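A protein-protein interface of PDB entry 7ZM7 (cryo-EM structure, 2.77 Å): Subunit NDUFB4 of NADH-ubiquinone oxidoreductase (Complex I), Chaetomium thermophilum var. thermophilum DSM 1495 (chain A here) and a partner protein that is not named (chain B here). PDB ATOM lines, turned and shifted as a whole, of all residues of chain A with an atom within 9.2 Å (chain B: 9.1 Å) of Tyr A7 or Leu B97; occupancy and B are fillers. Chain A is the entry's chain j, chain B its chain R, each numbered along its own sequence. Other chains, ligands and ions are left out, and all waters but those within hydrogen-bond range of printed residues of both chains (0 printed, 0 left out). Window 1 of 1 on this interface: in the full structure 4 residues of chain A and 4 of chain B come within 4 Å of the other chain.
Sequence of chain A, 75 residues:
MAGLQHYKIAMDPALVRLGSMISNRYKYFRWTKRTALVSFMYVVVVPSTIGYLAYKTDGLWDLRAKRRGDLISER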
ATOM      1  N   LEU A   4       8.995 -25.276  23.544  1.00  0.00           N
ATOM      2  CA  LEU A   4       8.608 -23.975  24.067  1.00  0.00           C
ATOM      3  C   LEU A   4       9.723 -22.967  23.845  1.00  0.00           C
ATOM      4  O   LEU A   4      10.906 -23.290  23.963  1.00  0.00           O
ATOM      5  CB  LEU A   4       8.292 -24.057  25.563  1.00  0.00           C
ATOM      6  CG  LEU A   4       6.879 -24.423  26.014  1.00  0.00           C
ATOM      7  CD1 LEU A   4       5.886 -23.409  25.469  1.00  0.00           C
ATOM      8  CD2 LEU A   4       6.524 -25.778  25.573  1.00  0.00           C
ATOM      9  N   GLN A   5       9.325 -21.724  23.590  1.00  0.00           N
ATOM     10  CA  GLN A   5      10.354 -20.665  23.508  1.00  0.00           C
ATOM     11  C   GLN A   5      10.744 -20.289  24.935  1.00  0.00           C
ATOM     12  O   GLN A   5       9.854 -20.060  25.762  1.00  0.00           O
ATOM     13  CB  GLN A   5       9.853 -19.461  22.710  1.00  0.00           C
ATOM     14  CG  GLN A   5       8.412 -19.074  23.007  1.00  0.00           C
ATOM     15  CD  GLN A   5       8.013 -17.818  22.272  1.00  0.00           C
ATOM     16  OE1 GLN A   5       8.841 -17.147  21.659  1.00  0.00           O
ATOM     17  NE2 GLN A   5       6.734 -17.489  22.332  1.00  0.00           N
ATOM     18  N   HIS A   6      12.040 -20.251  25.194  1.00  0.00           N
ATOM     19  CA  HIS A   6      12.573 -19.903  26.523  1.00  0.00           C
ATOM     20  C   HIS A   6      12.764 -18.384  26.621  1.00  0.00           C
ATOM     21  O   HIS A   6      12.521 -17.699  25.623  1.00  0.00           O
ATOM     22  CB  HIS A   6      13.854 -20.707  26.721  1.00  0.00           C
ATOM     23  CG  HIS A   6      14.859 -20.566  25.631  1.00  0.00           C
ATOM     24  ND1 HIS A   6      15.774 -19.539  25.600  1.00  0.00           N
ATOM     25  CD2 HIS A   6      15.119 -21.338  24.558  1.00  0.00           C
ATOM     26  CE1 HIS A   6      16.542 -19.668  24.543  1.00  0.00           C
ATOM     27  NE2 HIS A   6      16.163 -20.764  23.888  1.00  0.00           N
ATOM     28  N   TYR A   7      13.114 -17.896  27.804  1.00  0.00           N
ATOM     29  CA  TYR A   7      13.369 -16.462  28.015  1.00  0.00           C
ATOM     30  C   TYR A   7      14.712 -16.125  27.375  1.00  0.00           C
ATOM     31  O   TYR A   7      15.507 -17.032  27.132  1.00  0.00           O
ATOM     32  CB  TYR A   7      13.369 -16.147  29.506  1.00  0.00           C
ATOM     33  CG  TYR A   7      12.052 -16.257  30.228  1.00  0.00           C
ATOM     34  CD1 TYR A   7      11.126 -15.235  30.170  1.00  0.00           C
ATOM     35  CD2 TYR A   7      11.754 -17.353  31.018  1.00  0.00           C
ATOM     36  CE1 TYR A   7       9.921 -15.314  30.844  1.00  0.00           C
ATOM     37  CE2 TYR A   7      10.554 -17.448  31.701  1.00  0.00           C
ATOM     38  CZ  TYR A   7       9.632 -16.425  31.613  1.00  0.00           C
ATOM     39  OH  TYR A   7       8.441 -16.496  32.274  1.00  0.00           O
ATOM     40  N   LYS A   8      14.994 -14.839  27.186  1.00  0.00           N
ATOM     41  CA  LYS A   8      16.257 -14.412  26.532  1.00  0.00           C
ATOM     42  C   LYS A   8      17.466 -14.657  27.443  1.00  0.00           C
ATOM     43  O   LYS A   8      17.413 -14.258  28.607  1.00  0.00           O
ATOM     44  CB  LYS A   8      16.137 -12.953  26.088  1.00  0.00           C
ATOM     45  CG  LYS A   8      14.893 -12.642  25.267  1.00  0.00           C
ATOM     46  CD  LYS A   8      14.772 -11.184  24.888  1.00  0.00           C
ATOM     47  CE  LYS A   8      13.443 -10.855  24.243  1.00  0.00           C
ATOM     48  NZ  LYS A   8      13.169 -11.728  23.077  1.00  0.00           N
ATOM     49  N   ILE A   9      18.506 -15.309  26.918  1.00  0.00           N
ATOM     50  CA  ILE A   9      19.747 -15.614  27.695  1.00  0.00           C
ATOM     51  C   ILE A   9      20.928 -14.998  26.958  1.00  0.00           C
ATOM     52  O   ILE A   9      20.990 -15.166  25.735  1.00  0.00           O
ATOM     53  CB  ILE A   9      19.949 -17.136  27.833  1.00  0.00           C
ATOM     54  CG1 ILE A   9      18.765 -17.799  28.533  1.00  0.00           C
ATOM     55  CG2 ILE A   9      21.247 -17.434  28.567  1.00  0.00           C
ATOM     56  CD1 ILE A   9      18.745 -17.542  30.014  1.00  0.00           C
ATOM     57  N   ALA A  10      21.784 -14.261  27.657  1.00  0.00           N
ATOM     58  CA  ALA A  10      23.015 -13.740  27.031  1.00  0.00           C
ATOM     59  C   ALA A  10      23.943 -14.928  26.844  1.00  0.00           C
ATOM     60  O   ALA A  10      24.882 -15.059  27.640  1.00  0.00           O
ATOM     61  CB  ALA A  10      23.668 -12.753  27.952  1.00  0.00           C
ATOM     62  N   MET A  11      23.658 -15.772  25.855  1.00  0.00           N
ATOM     63  CA  MET A  11      24.468 -16.986  25.697  1.00  0.00           C
ATOM     64  C   MET A  11      25.886 -16.507  25.443  1.00  0.00           C
ATOM     65  O   MET A  11      26.080 -15.661  24.553  1.00  0.00           O
ATOM     66  CB  MET A  11      23.942 -17.802  24.523  1.00  0.00           C
ATOM     67  CG  MET A  11      23.819 -19.282  24.838  1.00  0.00           C
ATOM     68  SD  MET A  11      22.967 -19.612  26.404  1.00  0.00           S
ATOM     69  CE  MET A  11      23.060 -21.400  26.467  1.00  0.00           C
ATOM     70  N   GLU B  92      12.290  -5.586  36.359  1.00  0.00           N
ATOM     71  CA  GLU B  92      11.139  -5.565  35.483  1.00  0.00           C
ATOM     72  C   GLU B  92      10.396  -6.895  35.557  1.00  0.00           C
ATOM     73  O   GLU B  92      11.008  -7.949  35.754  1.00  0.00           O
ATOM     74  CB  GLU B  92      11.555  -5.275  34.046  1.00  0.00           C
ATOM     75  CG  GLU B  92      12.032  -3.855  33.813  1.00  0.00           C
ATOM     76  CD  GLU B  92      13.483  -3.635  34.193  1.00  0.00           C
ATOM     77  OE1 GLU B  92      14.157  -4.608  34.590  1.00  0.00           O
ATOM     78  OE2 GLU B  92      13.952  -2.481  34.094  1.00  0.00           O
ATOM     79  N   PRO B  93       9.037  -6.889  35.483  1.00  0.00           N
ATOM     80  CA  PRO B  93       8.281  -8.128  35.439  1.00  0.00           C
ATOM     81  C   PRO B  93       8.814  -8.960  34.271  1.00  0.00           C
ATOM     82  O   PRO B  93       9.265  -8.390  33.300  1.00  0.00           O
ATOM     83  CB  PRO B  93       6.882  -7.645  35.070  1.00  0.00           C
ATOM     84  CG  PRO B  93       6.760  -6.353  35.809  1.00  0.00           C
ATOM     85  CD  PRO B  93       8.110  -5.729  35.547  1.00  0.00           C
ATOM     86  N   PRO B  94       8.724 -10.303  34.327  1.00  0.00           N
ATOM     87  CA  PRO B  94       9.270 -11.141  33.269  1.00  0.00           C
ATOM     88  C   PRO B  94       8.396 -11.015  32.010  1.00  0.00           C
ATOM     89  O   PRO B  94       7.250 -10.650  32.138  1.00  0.00           O
ATOM     90  CB  PRO B  94       9.210 -12.545  33.896  1.00  0.00           C
ATOM     91  CG  PRO B  94       8.853 -12.342  35.347  1.00  0.00           C
ATOM     92  CD  PRO B  94       8.046 -11.067  35.364  1.00  0.00           C
ATOM     93  N   PRO B  95       8.888 -11.311  30.788  1.00  0.00           N
ATOM     94  CA  PRO B  95       8.008 -11.251  29.615  1.00  0.00           C
ATOM     95  C   PRO B  95       7.036 -12.443  29.611  1.00  0.00           C
ATOM     96  O   PRO B  95       7.463 -13.522  29.946  1.00  0.00           O
ATOM     97  CB  PRO B  95       8.973 -11.391  28.440  1.00  0.00           C
ATOM     98  CG  PRO B  95      10.196 -12.056  29.026  1.00  0.00           C
ATOM     99  CD  PRO B  95      10.280 -11.597  30.465  1.00  0.00           C
ATOM    100  N   PRO B  96       5.741 -12.308  29.224  1.00  0.00           N
ATOM    101  CA  PRO B  96       4.771 -13.396  29.411  1.00  0.00           C
ATOM    102  C   PRO B  96       5.063 -14.632  28.574  1.00  0.00           C
ATOM    103  O   PRO B  96       4.871 -14.632  27.357  1.00  0.00           O
ATOM    104  CB  PRO B  96       3.446 -12.749  28.995  1.00  0.00           C
ATOM    105  CG  PRO B  96       3.829 -11.641  28.115  1.00  0.00           C
ATOM    106  CD  PRO B  96       5.121 -11.117  28.628  1.00  0.00           C
ATOM    107  N   LEU B  97       5.515 -15.700  29.223  1.00  0.00           N
ATOM    108  CA  LEU B  97       5.788 -16.960  28.553  1.00  0.00           C
ATOM    109  C   LEU B  97       5.195 -18.112  29.356  1.00  0.00           C
ATOM    110  O   LEU B  97       5.346 -18.174  30.576  1.00  0.00           O
ATOM    111  CB  LEU B  97       7.294 -17.159  28.354  1.00  0.00           C
ATOM    112  CG  LEU B  97       7.945 -16.288  27.285  1.00  0.00           C
ATOM    113  CD1 LEU B  97       9.413 -16.464  27.309  1.00  0.00           C
ATOM    114  CD2 LEU B  97       7.399 -16.655  25.925  1.00  0.00           C
ATOM    115  N   LYS B  98       4.536 -19.032  28.657  1.00  0.00           N
ATOM    116  CA  LYS B  98       3.823 -20.138  29.277  1.00  0.00           C
ATOM    117  C   LYS B  98       4.742 -21.328  29.510  1.00  0.00           C
ATOM    118  O   LYS B  98       5.605 -21.632  28.685  1.00  0.00           O
ATOM    119  CB  LYS B  98       2.648 -20.563  28.396  1.00  0.00           C
ATOM    120  CG  LYS B  98       1.614 -19.480  28.176  1.00  0.00           C
ATOM    121  CD  LYS B  98       0.983 -19.063  29.487  1.00  0.00           C
ATOM    122  CE  LYS B  98       0.159 -20.194  30.070  1.00  0.00           C
ATOM    123  NZ  LYS B  98      -0.999 -20.520  29.195  1.00  0.00           N
ATOM    124  N   PHE B  99       4.532 -22.017  30.627  1.00  0.00           N
ATOM    125  CA  PHE B  99       5.385 -23.144  30.991  1.00  0.00           C
ATOM    126  C   PHE B  99       4.636 -24.290  31.655  1.00  0.00           C
ATOM    127  O   PHE B  99       4.933 -25.455  31.396  1.00  0.00           O
ATOM    128  CB  PHE B  99       6.519 -22.670  31.902  1.00  0.00           C
ATOM    129  CG  PHE B  99       7.536 -21.863  31.188  1.00  0.00           C
ATOM    130  CD1 PHE B  99       8.199 -22.391  30.103  1.00  0.00           C
ATOM    131  CD2 PHE B  99       7.798 -20.561  31.559  1.00  0.00           C
ATOM    132  CE1 PHE B  99       9.121 -21.646  29.423  1.00  0.00           C
ATOM    133  CE2 PHE B  99       8.728 -19.818  30.877  1.00  0.00           C
ATOM    134  CZ  PHE B  99       9.390 -20.361  29.812  1.00  0.00           C
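Hydrophobic or aromatic side chains of chain B that line the printed part of chain A: Pro B95, Leu B97 and Phe B99. Of the 8 printed residues of chain A, 4 touch a printed residue of chain B. Hydrophobic or aromatic side chains of chain A that line the printed part of chain B: Leu A4 and Tyr A7. Along chain A the printed residues that touch a printed residue of chain B span positions 4 to 7. Among the printed residues, 6 pairs touch across the chains.
Of the printed residues of chain B, Leu A4 touches Lys B98 (3.7 Å). Of the printed residues of chain B, Gln A5 touches Leu B97 (3.7 Å). Of chain B, only Pro B95 (3.2 Å), Leu B97 (3.6 Å) and Phe B99 (3.1 Å) come within 4 Å of Tyr A7. Glu B92 touches none of the printed residues of chain A. Pro B93 touches none of the printed residues of chain A. Pro B95 touches just one residue of chain A: Tyr A7 (3.2 Å). Pro B96 touches none of the printed residues of chain A. Printed residues of chain A within 4 Å of Lys B98: Leu A4 (3.7 Å). The nearest residue of chain B that does not touch Tyr A7 is Pro B94 (4.2 Å). The nearest printed residue of chain B that does not touch Gln A5 is Phe B99 (4.1 Å).
Among the printed residues, pairs that only touch across the chains: Leu A4 with Lys B98 (3.7 Å), Gln A5 with Leu B97 (3.7 Å), His A6 with Leu B97 (3.7 Å), Tyr A7 with Pro B95 (3.2 Å), Tyr A7 with Leu B97 (3.6 Å) and Tyr A7 with Phe B99 (3.1 Å).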
